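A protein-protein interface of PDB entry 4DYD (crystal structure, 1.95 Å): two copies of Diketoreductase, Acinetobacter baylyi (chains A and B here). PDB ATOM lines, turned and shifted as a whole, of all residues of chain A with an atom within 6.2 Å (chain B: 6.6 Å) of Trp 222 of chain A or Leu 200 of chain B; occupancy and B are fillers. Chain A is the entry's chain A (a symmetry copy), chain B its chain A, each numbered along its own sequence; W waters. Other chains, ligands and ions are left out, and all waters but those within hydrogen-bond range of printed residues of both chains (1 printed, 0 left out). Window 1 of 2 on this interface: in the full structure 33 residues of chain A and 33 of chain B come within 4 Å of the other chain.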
ATOM      1  N   LEU A 196      -5.269 -15.797  26.193  1.00  0.00           N
ATOM      2  CA  LEU A 196      -6.153 -14.698  25.770  1.00  0.00           C
ATOM      3  C   LEU A 196      -7.616 -14.983  26.087  1.00  0.00           C
ATOM      4  O   LEU A 196      -8.350 -14.094  26.530  1.00  0.00           O
ATOM      5  CB  LEU A 196      -6.019 -14.440  24.260  1.00  0.00           C
ATOM      6  CG  LEU A 196      -4.663 -13.964  23.740  1.00  0.00           C
ATOM      7  CD1 LEU A 196      -4.678 -13.876  22.214  1.00  0.00           C
ATOM      8  CD2 LEU A 196      -4.316 -12.615  24.370  1.00  0.00           C
ATOM      9  N   LEU A 197      -8.035 -16.222  25.849  1.00  0.00           N
ATOM     10  CA  LEU A 197      -9.446 -16.590  25.910  1.00  0.00           C
ATOM     11  C   LEU A 197      -9.996 -16.713  27.332  1.00  0.00           C
ATOM     12  O   LEU A 197     -11.113 -16.269  27.609  1.00  0.00           O
ATOM     13  CB  LEU A 197      -9.682 -17.897  25.151  1.00  0.00           C
ATOM     14  CG  LEU A 197     -11.132 -18.388  25.084  1.00  0.00           C
ATOM     15  CD1 LEU A 197     -11.988 -17.362  24.353  1.00  0.00           C
ATOM     16  CD2 LEU A 197     -11.190 -19.734  24.377  1.00  0.00           C
ATOM     17  N   PRO A 199      -9.301 -15.197  30.157  1.00  0.00           N
ATOM     18  CA  PRO A 199      -9.691 -13.942  30.809  1.00  0.00           C
ATOM     19  C   PRO A 199     -11.008 -13.378  30.257  1.00  0.00           C
ATOM     20  O   PRO A 199     -11.815 -12.818  31.005  1.00  0.00           O
ATOM     21  CB  PRO A 199      -8.514 -13.010  30.508  1.00  0.00           C
ATOM     22  CG  PRO A 199      -7.354 -13.938  30.292  1.00  0.00           C
ATOM     23  CD  PRO A 199      -7.936 -15.133  29.601  1.00  0.00           C
ATOM     24  N   LEU A 200     -11.234 -13.526  28.955  1.00  0.00           N
ATOM     25  CA  LEU A 200     -12.497 -13.085  28.364  1.00  0.00           C
ATOM     26  C   LEU A 200     -13.675 -13.893  28.920  1.00  0.00           C
ATOM     27  O   LEU A 200     -14.686 -13.326  29.343  1.00  0.00           O
ATOM     28  CB  LEU A 200     -12.465 -13.196  26.833  1.00  0.00           C
ATOM     29  CG  LEU A 200     -13.779 -12.847  26.116  1.00  0.00           C
ATOM     30  CD1 LEU A 200     -14.223 -11.422  26.445  1.00  0.00           C
ATOM     31  CD2 LEU A 200     -13.634 -13.035  24.608  1.00  0.00           C
ATOM     32  N   THR A 217     -27.353 -10.728  26.348  1.00  0.00           N
ATOM     33  CA  THR A 217     -26.931  -9.338  26.400  1.00  0.00           C
ATOM     34  C   THR A 217     -25.421  -9.239  26.351  1.00  0.00           C
ATOM     35  O   THR A 217     -24.864  -8.395  25.642  1.00  0.00           O
ATOM     36  CB  THR A 217     -27.445  -8.658  27.678  1.00  0.00           C
ATOM     37  OG1 THR A 217     -28.875  -8.605  27.632  1.00  0.00           O
ATOM     38  CG2 THR A 217     -26.886  -7.252  27.812  1.00  0.00           C
ATOM     39  N   ILE A 218     -24.761 -10.104  27.113  1.00  0.00           N
ATOM     40  CA  ILE A 218     -23.311 -10.117  27.164  1.00  0.00           C
ATOM     41  C   ILE A 218     -22.733 -10.451  25.791  1.00  0.00           C
ATOM     42  O   ILE A 218     -21.796  -9.794  25.330  1.00  0.00           O
ATOM     43  CB  ILE A 218     -22.796 -11.109  28.236  1.00  0.00           C
ATOM     44  CG1 ILE A 218     -23.238 -10.644  29.634  1.00  0.00           C
ATOM     45  CG2 ILE A 218     -21.287 -11.243  28.148  1.00  0.00           C
ATOM     46  CD1 ILE A 218     -22.852 -11.581  30.775  1.00  0.00           C
ATOM     47  N   ASP A 219     -23.298 -11.464  25.141  1.00  0.00           N
ATOM     48  CA  ASP A 219     -22.833 -11.870  23.822  1.00  0.00           C
ATOM     49  C   ASP A 219     -23.024 -10.802  22.752  1.00  0.00           C
ATOM     50  O   ASP A 219     -22.090 -10.523  21.995  1.00  0.00           O
ATOM     51  CB  ASP A 219     -23.461 -13.193  23.389  1.00  0.00           C
ATOM     52  CG  ASP A 219     -22.856 -14.388  24.105  1.00  0.00           C
ATOM     53  OD1 ASP A 219     -21.856 -14.205  24.830  1.00  0.00           O
ATOM     54  OD2 ASP A 219     -23.367 -15.514  23.932  1.00  0.00           O
ATOM     55  N   LYS A 220     -24.210 -10.204  22.669  1.00  0.00           N
ATOM     56  CA  LYS A 220     -24.421  -9.197  21.634  1.00  0.00           C
ATOM     57  C   LYS A 220     -23.514  -7.990  21.854  1.00  0.00           C
ATOM     58  O   LYS A 220     -23.063  -7.368  20.890  1.00  0.00           O
ATOM     59  CB  LYS A 220     -25.893  -8.787  21.498  1.00  0.00           C
ATOM     60  CG  LYS A 220     -26.519  -8.125  22.706  1.00  0.00           C
ATOM     61  CD  LYS A 220     -27.979  -7.797  22.409  1.00  0.00           C
ATOM     62  CE  LYS A 220     -28.684  -7.167  23.599  1.00  0.00           C
ATOM     63  NZ  LYS A 220     -30.115  -6.876  23.293  1.00  0.00           N
ATOM     64  N   THR A 221     -23.226  -7.674  23.115  1.00  0.00           N
ATOM     65  CA  THR A 221     -22.316  -6.583  23.433  1.00  0.00           C
ATOM     66  C   THR A 221     -20.933  -6.864  22.853  1.00  0.00           C
ATOM     67  O   THR A 221     -20.287  -5.972  22.297  1.00  0.00           O
ATOM     68  CB  THR A 221     -22.192  -6.376  24.958  1.00  0.00           C
ATOM     69  OG1 THR A 221     -23.480  -6.085  25.503  1.00  0.00           O
ATOM     70  CG2 THR A 221     -21.257  -5.222  25.269  1.00  0.00           C
ATOM     71  N   TRP A 222     -20.475  -8.105  22.973  1.00  0.00           N
ATOM     72  CA  TRP A 222     -19.156  -8.461  22.466  1.00  0.00           C
ATOM     73  C   TRP A 222     -19.141  -8.461  20.933  1.00  0.00           C
ATOM     74  O   TRP A 222     -18.187  -7.978  20.317  1.00  0.00           O
ATOM     75  CB  TRP A 222     -18.721  -9.834  22.980  1.00  0.00           C
ATOM     76  CG  TRP A 222     -17.294 -10.163  22.635  1.00  0.00           C
ATOM     77  CD1 TRP A 222     -16.853 -11.125  21.764  1.00  0.00           C
ATOM     78  CD2 TRP A 222     -16.116  -9.525  23.155  1.00  0.00           C
ATOM     79  NE1 TRP A 222     -15.476 -11.124  21.713  1.00  0.00           N
ATOM     80  CE2 TRP A 222     -14.999 -10.151  22.555  1.00  0.00           C
ATOM     81  CE3 TRP A 222     -15.898  -8.483  24.070  1.00  0.00           C
ATOM     82  CZ2 TRP A 222     -13.683  -9.772  22.839  1.00  0.00           C
ATOM     83  CZ3 TRP A 222     -14.588  -8.103  24.354  1.00  0.00           C
ATOM     84  CH2 TRP A 222     -13.497  -8.749  23.738  1.00  0.00           C
ATOM     85  N   ARG A 223     -20.187  -9.008  20.316  1.00  0.00           N
ATOM     86  CA  ARG A 223     -20.231  -9.050  18.855  1.00  0.00           C
ATOM     87  C   ARG A 223     -20.278  -7.643  18.264  1.00  0.00           C
ATOM     88  O   ARG A 223     -19.559  -7.341  17.309  1.00  0.00           O
ATOM     89  CB  ARG A 223     -21.400  -9.894  18.336  1.00  0.00           C
ATOM     90  CG  ARG A 223     -21.327 -11.377  18.704  1.00  0.00           C
ATOM     91  CD  ARG A 223     -22.351 -12.193  17.909  1.00  0.00           C
ATOM     92  NE  ARG A 223     -23.698 -11.654  18.078  1.00  0.00           N
ATOM     93  CZ  ARG A 223     -24.569 -12.072  18.991  1.00  0.00           C
ATOM     94  NH1 ARG A 223     -24.247 -13.049  19.827  1.00  0.00           N
ATOM     95  NH2 ARG A 223     -25.769 -11.509  19.075  1.00  0.00           N
ATOM     96  N   ILE A 224     -21.106  -6.780  18.840  1.00  0.00           N
ATOM     97  CA  ILE A 224     -21.236  -5.414  18.341  1.00  0.00           C
ATOM     98  C   ILE A 224     -20.014  -4.577  18.683  1.00  0.00           C
ATOM     99  O   ILE A 224     -19.543  -3.783  17.863  1.00  0.00           O
ATOM    100  CB  ILE A 224     -22.485  -4.722  18.901  1.00  0.00           C
ATOM    101  CG1 ILE A 224     -23.741  -5.435  18.396  1.00  0.00           C
ATOM    102  CG2 ILE A 224     -22.493  -3.252  18.508  1.00  0.00           C
ATOM    103  CD1 ILE A 224     -25.031  -4.841  18.903  1.00  0.00           C
ATOM    104  N   GLY A 225     -19.499  -4.756  19.893  1.00  0.00           N
ATOM    105  CA  GLY A 225     -18.375  -3.957  20.337  1.00  0.00           C
ATOM    106  C   GLY A 225     -17.064  -4.266  19.644  1.00  0.00           C
ATOM    107  O   GLY A 225     -16.236  -3.373  19.461  1.00  0.00           O
ATOM    108  N   THR A 226     -16.861  -5.519  19.251  1.00  0.00           N
ATOM    109  CA  THR A 226     -15.582  -5.907  18.669  1.00  0.00           C
ATOM    110  C   THR A 226     -15.732  -6.449  17.251  1.00  0.00           C
ATOM    111  O   THR A 226     -14.734  -6.733  16.584  1.00  0.00           O
ATOM    112  CB  THR A 226     -14.895  -6.996  19.505  1.00  0.00           C
ATOM    113  OG1 THR A 226     -15.702  -8.180  19.494  1.00  0.00           O
ATOM    114  CG2 THR A 226     -14.694  -6.520  20.940  1.00  0.00           C
ATOM    115  N   GLY A 227     -16.969  -6.609  16.795  1.00  0.00           N
ATOM    116  CA  GLY A 227     -17.185  -7.205  15.492  1.00  0.00           C
ATOM    117  C   GLY A 227     -16.956  -8.704  15.465  1.00  0.00           C
ATOM    118  O   GLY A 227     -16.971  -9.321  14.399  1.00  0.00           O
ATOM    119  N   ALA A 228     -16.752  -9.301  16.634  1.00  0.00           N
ATOM    120  CA  ALA A 228     -16.542 -10.743  16.721  1.00  0.00           C
ATOM    121  C   ALA A 228     -17.795 -11.496  16.270  1.00  0.00           C
ATOM    122  O   ALA A 228     -18.919 -11.047  16.507  1.00  0.00           O
ATOM    123  CB  ALA A 228     -16.168 -11.143  18.144  1.00  0.00           C
ATOM    124  N   LYS A 230     -18.774 -14.513  17.344  1.00  0.00           N
ATOM    125  CA  LYS A 230     -19.410 -15.205  18.459  1.00  0.00           C
ATOM    126  C   LYS A 230     -19.075 -14.585  19.814  1.00  0.00           C
ATOM    127  O   LYS A 230     -17.933 -14.190  20.068  1.00  0.00           O
ATOM    128  CB  LYS A 230     -19.068 -16.695  18.427  1.00  0.00           C
ATOM    129  CG  LYS A 230     -19.615 -17.383  17.184  1.00  0.00           C
ATOM    130  CD  LYS A 230     -19.274 -18.852  17.130  1.00  0.00           C
ATOM    131  CE  LYS A 230     -19.854 -19.476  15.864  1.00  0.00           C
ATOM    132  NZ  LYS A 230     -21.336 -19.289  15.806  1.00  0.00           N
ATOM    133  N   GLY A 231     -20.088 -14.499  20.673  1.00  0.00           N
ATOM    134  CA  GLY A 231     -19.892 -13.977  22.013  1.00  0.00           C
ATOM    135  C   GLY A 231     -19.351 -15.017  22.977  1.00  0.00           C
ATOM    136  O   GLY A 231     -19.288 -16.201  22.636  1.00  0.00           O
ATOM    137  N   PRO A 232     -18.950 -14.615  24.191  1.00  0.00           N
ATOM    138  CA  PRO A 232     -18.409 -15.562  25.178  1.00  0.00           C
ATOM    139  C   PRO A 232     -19.257 -16.807  25.431  1.00  0.00           C
ATOM    140  O   PRO A 232     -18.731 -17.920  25.505  1.00  0.00           O
ATOM    141  CB  PRO A 232     -18.269 -14.714  26.440  1.00  0.00           C
ATOM    142  CG  PRO A 232     -18.098 -13.315  25.920  1.00  0.00           C
ATOM    143  CD  PRO A 232     -18.988 -13.236  24.711  1.00  0.00           C
ATOM    144  N   ILE A 235     -19.254 -19.169  22.729  1.00  0.00           N
ATOM    145  CA  ILE A 235     -17.965 -19.842  22.838  1.00  0.00           C
ATOM    146  C   ILE A 235     -17.994 -20.933  23.901  1.00  0.00           C
ATOM    147  O   ILE A 235     -17.447 -22.017  23.687  1.00  0.00           O
ATOM    148  CB  ILE A 235     -16.823 -18.840  23.099  1.00  0.00           C
ATOM    149  CG1 ILE A 235     -16.687 -17.898  21.896  1.00  0.00           C
ATOM    150  CG2 ILE A 235     -15.520 -19.577  23.370  1.00  0.00           C
ATOM    151  CD1 ILE A 235     -15.606 -16.837  22.033  1.00  0.00           C
ATOM    152  N   VAL B 192     -20.688  -3.499  30.572  1.00  0.00           N
ATOM    153  CA  VAL B 192     -20.432  -4.810  29.972  1.00  0.00           C
ATOM    154  C   VAL B 192     -19.210  -4.823  29.053  1.00  0.00           C
ATOM    155  O   VAL B 192     -18.271  -5.594  29.273  1.00  0.00           O
ATOM    156  CB  VAL B 192     -21.655  -5.354  29.208  1.00  0.00           C
ATOM    157  CG1 VAL B 192     -21.308  -6.687  28.550  1.00  0.00           C
ATOM    158  CG2 VAL B 192     -22.840  -5.523  30.158  1.00  0.00           C
ATOM    159  N   LEU B 193     -19.222  -3.980  28.021  1.00  0.00           N
ATOM    160  CA  LEU B 193     -18.162  -4.013  27.015  1.00  0.00           C
ATOM    161  C   LEU B 193     -16.752  -3.873  27.593  1.00  0.00           C
ATOM    162  O   LEU B 193     -15.882  -4.703  27.316  1.00  0.00           O
ATOM    163  CB  LEU B 193     -18.396  -2.971  25.915  1.00  0.00           C
ATOM    164  CG  LEU B 193     -17.291  -2.928  24.855  1.00  0.00           C
ATOM    165  CD1 LEU B 193     -17.002  -4.320  24.307  1.00  0.00           C
ATOM    166  CD2 LEU B 193     -17.655  -1.955  23.744  1.00  0.00           C
ATOM    167  N   SER B 195     -15.797  -4.251  30.628  1.00  0.00           N
ATOM    168  CA  SER B 195     -15.592  -5.397  31.508  1.00  0.00           C
ATOM    169  C   SER B 195     -15.080  -6.615  30.740  1.00  0.00           C
ATOM    170  O   SER B 195     -14.303  -7.406  31.276  1.00  0.00           O
ATOM    171  CB  SER B 195     -16.882  -5.748  32.251  1.00  0.00           C
ATOM    172  OG  SER B 195     -17.288  -4.688  33.101  1.00  0.00           O
ATOM    173  N   LEU B 196     -15.513  -6.776  29.491  1.00  0.00           N
ATOM    174  CA  LEU B 196     -15.062  -7.913  28.670  1.00  0.00           C
ATOM    175  C   LEU B 196     -13.724  -7.638  27.995  1.00  0.00           C
ATOM    176  O   LEU B 196     -12.857  -8.516  27.933  1.00  0.00           O
ATOM    177  CB  LEU B 196     -16.100  -8.248  27.587  1.00  0.00           C
ATOM    178  CG  LEU B 196     -17.476  -8.726  28.048  1.00  0.00           C
ATOM    179  CD1 LEU B 196     -18.410  -8.896  26.849  1.00  0.00           C
ATOM    180  CD2 LEU B 196     -17.331 -10.032  28.828  1.00  0.00           C
ATOM    181  N   LEU B 197     -13.567  -6.421  27.482  1.00  0.00           N
ATOM    182  CA  LEU B 197     -12.431  -6.077  26.633  1.00  0.00           C
ATOM    183  C   LEU B 197     -11.118  -5.889  27.397  1.00  0.00           C
ATOM    184  O   LEU B 197     -10.062  -6.338  26.944  1.00  0.00           O
ATOM    185  CB  LEU B 197     -12.741  -4.818  25.823  1.00  0.00           C
ATOM    186  CG  LEU B 197     -11.656  -4.358  24.844  1.00  0.00           C
ATOM    187  CD1 LEU B 197     -11.419  -5.438  23.796  1.00  0.00           C
ATOM    188  CD2 LEU B 197     -12.074  -3.053  24.183  1.00  0.00           C
ATOM    189  N   VAL B 198     -11.172  -5.216  28.540  1.00  0.00           N
ATOM    190  CA  VAL B 198      -9.955  -4.924  29.294  1.00  0.00           C
ATOM    191  C   VAL B 198      -9.182  -6.193  29.652  1.00  0.00           C
ATOM    192  O   VAL B 198      -7.956  -6.241  29.520  1.00  0.00           O
ATOM    193  CB  VAL B 198     -10.258  -4.087  30.553  1.00  0.00           C
ATOM    194  CG1 VAL B 198      -9.002  -3.929  31.398  1.00  0.00           C
ATOM    195  CG2 VAL B 198     -10.794  -2.722  30.138  1.00  0.00           C
ATOM    196  N   PRO B 199      -9.881  -7.238  30.119  1.00  0.00           N
ATOM    197  CA  PRO B 199      -9.146  -8.462  30.454  1.00  0.00           C
ATOM    198  C   PRO B 199      -8.446  -9.081  29.236  1.00  0.00           C
ATOM    199  O   PRO B 199      -7.339  -9.614  29.348  1.00  0.00           O
ATOM    200  CB  PRO B 199     -10.238  -9.388  31.000  1.00  0.00           C
ATOM    201  CG  PRO B 199     -11.298  -8.451  31.501  1.00  0.00           C
ATOM    202  CD  PRO B 199     -11.294  -7.306  30.535  1.00  0.00           C
ATOM    203  N   LEU B 200      -9.081  -9.006  28.069  1.00  0.00           N
ATOM    204  CA  LEU B 200      -8.449  -9.502  26.846  1.00  0.00           C
ATOM    205  C   LEU B 200      -7.197  -8.687  26.506  1.00  0.00           C
ATOM    206  O   LEU B 200      -6.130  -9.250  26.239  1.00  0.00           O
ATOM    207  CB  LEU B 200      -9.427  -9.473  25.663  1.00  0.00           C
ATOM    208  CG  LEU B 200      -8.837  -9.884  24.305  1.00  0.00           C
ATOM    209  CD1 LEU B 200      -8.258 -11.297  24.363  1.00  0.00           C
ATOM    210  CD2 LEU B 200      -9.890  -9.775  23.205  1.00  0.00           C
ATOM    211  N   LEU B 201      -7.332  -7.364  26.519  1.00  0.00           N
ATOM    212  CA  LEU B 201      -6.211  -6.495  26.183  1.00  0.00           C
ATOM    213  C   LEU B 201      -5.102  -6.588  27.233  1.00  0.00           C
ATOM    214  O   LEU B 201      -3.918  -6.523  26.887  1.00  0.00           O
ATOM    215  CB  LEU B 201      -6.667  -5.046  25.998  1.00  0.00           C
ATOM    216  CG  LEU B 201      -7.719  -4.789  24.910  1.00  0.00           C
ATOM    217  CD1 LEU B 201      -8.030  -3.301  24.837  1.00  0.00           C
ATOM    218  CD2 LEU B 201      -7.227  -5.288  23.559  1.00  0.00           C
ATOM    219  N   ASP B 202      -5.475  -6.744  28.503  1.00  0.00           N
ATOM    220  CA  ASP B 202      -4.474  -6.963  29.560  1.00  0.00           C
ATOM    221  C   ASP B 202      -3.674  -8.237  29.332  1.00  0.00           C
ATOM    222  O   ASP B 202      -2.452  -8.249  29.512  1.00  0.00           O
ATOM    223  CB  ASP B 202      -5.107  -7.046  30.952  1.00  0.00           C
ATOM    224  CG  ASP B 202      -5.628  -5.719  31.446  1.00  0.00           C
ATOM    225  OD1 ASP B 202      -5.303  -4.684  30.831  1.00  0.00           O
ATOM    226  OD2 ASP B 202      -6.360  -5.714  32.463  1.00  0.00           O
ATOM    227  N   ALA B 203      -4.359  -9.317  28.962  1.00  0.00           N
ATOM    228  CA  ALA B 203      -3.680 -10.592  28.745  1.00  0.00           C
ATOM    229  C   ALA B 203      -2.721 -10.476  27.559  1.00  0.00           C
ATOM    230  O   ALA B 203      -1.616 -11.023  27.579  1.00  0.00           O
ATOM    231  CB  ALA B 203      -4.693 -11.707  28.509  1.00  0.00           C
ATOM    232  N   ALA B 204      -3.142  -9.752  26.528  1.00  0.00           N
ATOM    233  CA  ALA B 204      -2.294  -9.544  25.359  1.00  0.00           C
ATOM    234  C   ALA B 204      -1.061  -8.729  25.757  1.00  0.00           C
ATOM    235  O   ALA B 204       0.064  -9.055  25.367  1.00  0.00           O
ATOM    236  CB  ALA B 204      -3.077  -8.829  24.254  1.00  0.00           C
ATOM    237  N   ALA B 205      -1.283  -7.672  26.530  1.00  0.00           N
ATOM    238  CA  ALA B 205      -0.196  -6.802  26.975  1.00  0.00           C
ATOM    239  C   ALA B 205       0.833  -7.596  27.781  1.00  0.00           C
ATOM    240  O   ALA B 205       2.041  -7.450  27.581  1.00  0.00           O
ATOM    241  CB  ALA B 205      -0.749  -5.655  27.803  1.00  0.00           C
ATOM    242  N   TRP B 222      -5.452 -14.912  17.943  1.00  0.00           N
ATOM    243  CA  TRP B 222      -6.808 -14.559  18.346  1.00  0.00           C
ATOM    244  C   TRP B 222      -7.772 -14.641  17.156  1.00  0.00           C
ATOM    245  O   TRP B 222      -8.893 -15.139  17.294  1.00  0.00           O
ATOM    246  CB  TRP B 222      -6.855 -13.153  18.945  1.00  0.00           C
ATOM    247  CG  TRP B 222      -8.194 -12.816  19.543  1.00  0.00           C
ATOM    248  CD1 TRP B 222      -9.098 -11.894  19.085  1.00  0.00           C
ATOM    249  CD2 TRP B 222      -8.782 -13.404  20.716  1.00  0.00           C
ATOM    250  NE1 TRP B 222     -10.209 -11.872  19.900  1.00  0.00           N
ATOM    251  CE2 TRP B 222     -10.042 -12.789  20.907  1.00  0.00           C
ATOM    252  CE3 TRP B 222      -8.365 -14.390  21.623  1.00  0.00           C
ATOM    253  CZ2 TRP B 222     -10.889 -13.128  21.966  1.00  0.00           C
ATOM    254  CZ3 TRP B 222      -9.208 -14.730  22.679  1.00  0.00           C
ATOM    255  CH2 TRP B 222     -10.458 -14.097  22.840  1.00  0.00           C
ATOM    256  N   ALA B 228     -12.329 -13.989  15.234  1.00  0.00           N
ATOM    257  CA  ALA B 228     -12.466 -12.540  15.355  1.00  0.00           C
ATOM    258  C   ALA B 228     -11.779 -11.836  14.184  1.00  0.00           C
ATOM    259  O   ALA B 228     -10.742 -12.292  13.695  1.00  0.00           O
ATOM    260  CB  ALA B 228     -11.883 -12.057  16.679  1.00  0.00           C
ATOM    261  N   LYS B 230     -10.401  -8.784  14.254  1.00  0.00           N
ATOM    262  CA  LYS B 230      -9.223  -8.045  14.694  1.00  0.00           C
ATOM    263  C   LYS B 230      -8.633  -8.585  15.994  1.00  0.00           C
ATOM    264  O   LYS B 230      -9.362  -8.946  16.923  1.00  0.00           O
ATOM    265  CB  LYS B 230      -9.539  -6.554  14.801  1.00  0.00           C
ATOM    266  CG  LYS B 230      -9.895  -5.943  13.453  1.00  0.00           C
ATOM    267  CD  LYS B 230     -10.223  -4.473  13.543  1.00  0.00           C
ATOM    268  CE  LYS B 230     -10.568  -3.929  12.160  1.00  0.00           C
ATOM    269  NZ  LYS B 230      -9.438  -4.147  11.204  1.00  0.00           N
ATOM    270  N   GLY B 231      -7.304  -8.645  16.041  1.00  0.00           N
ATOM    271  CA  GLY B 231      -6.616  -9.091  17.239  1.00  0.00           C
ATOM    272  C   GLY B 231      -6.461  -7.990  18.273  1.00  0.00           C
ATOM    273  O   GLY B 231      -6.744  -6.825  17.982  1.00  0.00           O
ATOM    274  N   PRO B 232      -6.013  -8.319  19.493  1.00  0.00           N
ATOM    275  CA  PRO B 232      -5.842  -7.310  20.551  1.00  0.00           C
ATOM    276  C   PRO B 232      -5.044  -6.069  20.155  1.00  0.00           C
ATOM    277  O   PRO B 232      -5.431  -4.945  20.479  1.00  0.00           O
ATOM    278  CB  PRO B 232      -5.152  -8.087  21.671  1.00  0.00           C
ATOM    279  CG  PRO B 232      -5.583  -9.508  21.445  1.00  0.00           C
ATOM    280  CD  PRO B 232      -5.635  -9.668  19.950  1.00  0.00           C
ATOM    281  N   ILE B 235      -6.767  -3.857  17.918  1.00  0.00           N
ATOM    282  CA  ILE B 235      -7.722  -3.154  18.766  1.00  0.00           C
ATOM    283  C   ILE B 235      -7.061  -2.009  19.521  1.00  0.00           C
ATOM    284  O   ILE B 235      -7.642  -0.927  19.635  1.00  0.00           O
ATOM    285  CB  ILE B 235      -8.436  -4.120  19.734  1.00  0.00           C
ATOM    286  CG1 ILE B 235      -9.273  -5.122  18.927  1.00  0.00           C
ATOM    287  CG2 ILE B 235      -9.304  -3.345  20.716  1.00  0.00           C
ATOM    288  CD1 ILE B 235     -10.014  -6.154  19.763  1.00  0.00           C
ATOM    289  N   PHE B 236      -5.850  -2.224  20.035  1.00  0.00           N
ATOM    290  CA  PHE B 236      -5.124  -1.126  20.681  1.00  0.00           C
ATOM    291  C   PHE B 236      -4.987   0.074  19.751  1.00  0.00           C
ATOM    292  O   PHE B 236      -5.219   1.217  20.161  1.00  0.00           O
ATOM    293  CB  PHE B 236      -3.733  -1.556  21.173  1.00  0.00           C
ATOM    294  CG  PHE B 236      -3.733  -2.216  22.526  1.00  0.00           C
ATOM    295  CD1 PHE B 236      -3.132  -3.458  22.715  1.00  0.00           C
ATOM    296  CD2 PHE B 236      -4.331  -1.590  23.615  1.00  0.00           C
ATOM    297  CE1 PHE B 236      -3.125  -4.069  23.976  1.00  0.00           C
ATOM    298  CE2 PHE B 236      -4.331  -2.192  24.884  1.00  0.00           C
ATOM    299  CZ  PHE B 236      -3.727  -3.434  25.059  1.00  0.00           C
HETATM  300  O   HOH W   1     -12.172  -8.492  16.856  1.00  0.00           O
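O of Thr 217 of chain A is in hydrogen-bond range of OG1 of Thr 221 of chain A (2.7 Å). The backbone carbonyl oxygen (O) of Trp 222 of chain A lies within hydrogen-bond range of the side-chain hydroxyl (OG1) of Thr 226 of chain A (2.6 Å).
Among the printed residues, pairs that only touch across the chains: Leu 196 of chain A with Leu 200 of chain B, Leu 196 of chain A with Ala 204 of chain B, Leu 196 of chain A with Trp 222 of chain B, Leu 197 of chain A with Trp 222 of chain B, Pro 199 of chain A with Pro 199 of chain B, Pro 199 of chain A with Ala 203 of chain B, Leu 200 of chain A with Leu 196 of chain B, Leu 200 of chain A with Trp 222 of chain B, Ile 218 of chain A with Leu 196 of chain B, Thr 221 of chain A with Val 192 of chain B, Thr 221 of chain A with Leu 193 of chain B, Trp 222 of chain A with Leu 196 of chain B, Trp 222 of chain A with Leu 197 of chain B and Trp 222 of chain A with Leu 200 of chain B.
Of the printed residues of chain B, Trp 222 of chain A touches Leu 196, Leu 197 and Leu 200. Leu 200 of chain B touches just these residues of chain A: Leu 196 and Trp 222. Printed residues of chain A within 4 Å of Leu 196 of chain B: Leu 200, Ile 218 and Trp 222. Of the printed residues of chain A, Ala 203 of chain B touches Pro 199 (3.9 Å). The nearest residue of chain A that does not touch Leu 200 of chain B is Pro 199 of chain A (4.7 Å). The nearest printed residue of chain A that does not touch Trp 222 of chain B is Trp 222 of chain A (4.5 Å).
Hydrophobic or aromatic side chains of chain B that line the printed part of chain A: Val 192, Leu 193, Leu 196, Leu 197, Pro 199, Leu 200, Ala 203, Ala 204 and Trp 222. Printed residues of chain A that touch a printed residue of chain B: Leu 196, Leu 197, Pro 199, Leu 200, Ile 218, Thr 221 and Trp 222. Hydrophobic or aromatic side chains of chain A within 4 Å of the printed part of chain B: Leu 196, Leu 197, Pro 199, Leu 200, Ile 218 and Trp 222. Among the printed residues, 14 pairs touch across the chains.
Leu 196 of chain A touches Trp 222 of chain B, and with the chains exchanged Trp 222 of chain A touches Leu 196 of chain B. Leu 197 of chain A touches Trp 222 of chain B, and with the chains exchanged Trp 222 of chain A touches Leu 197 of chain B. Pro 199 of chain A touches its own counterpart, Pro 199 of chain B. Leu 200 of chain A touches Trp 222 of chain B, and with the chains exchanged Trp 222 of chain A touches Leu 200 of chain B. Of the 14 pairs that touch across the chains among the printed residues, 9 have their exchanged pair printed and touching as well.
Water W1 lies within hydrogen-bond range of the backbone carbonyl oxygen (O) of Lys 230 of chain B and the backbone carbonyl oxygen (O) of Thr 226 of chain A.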
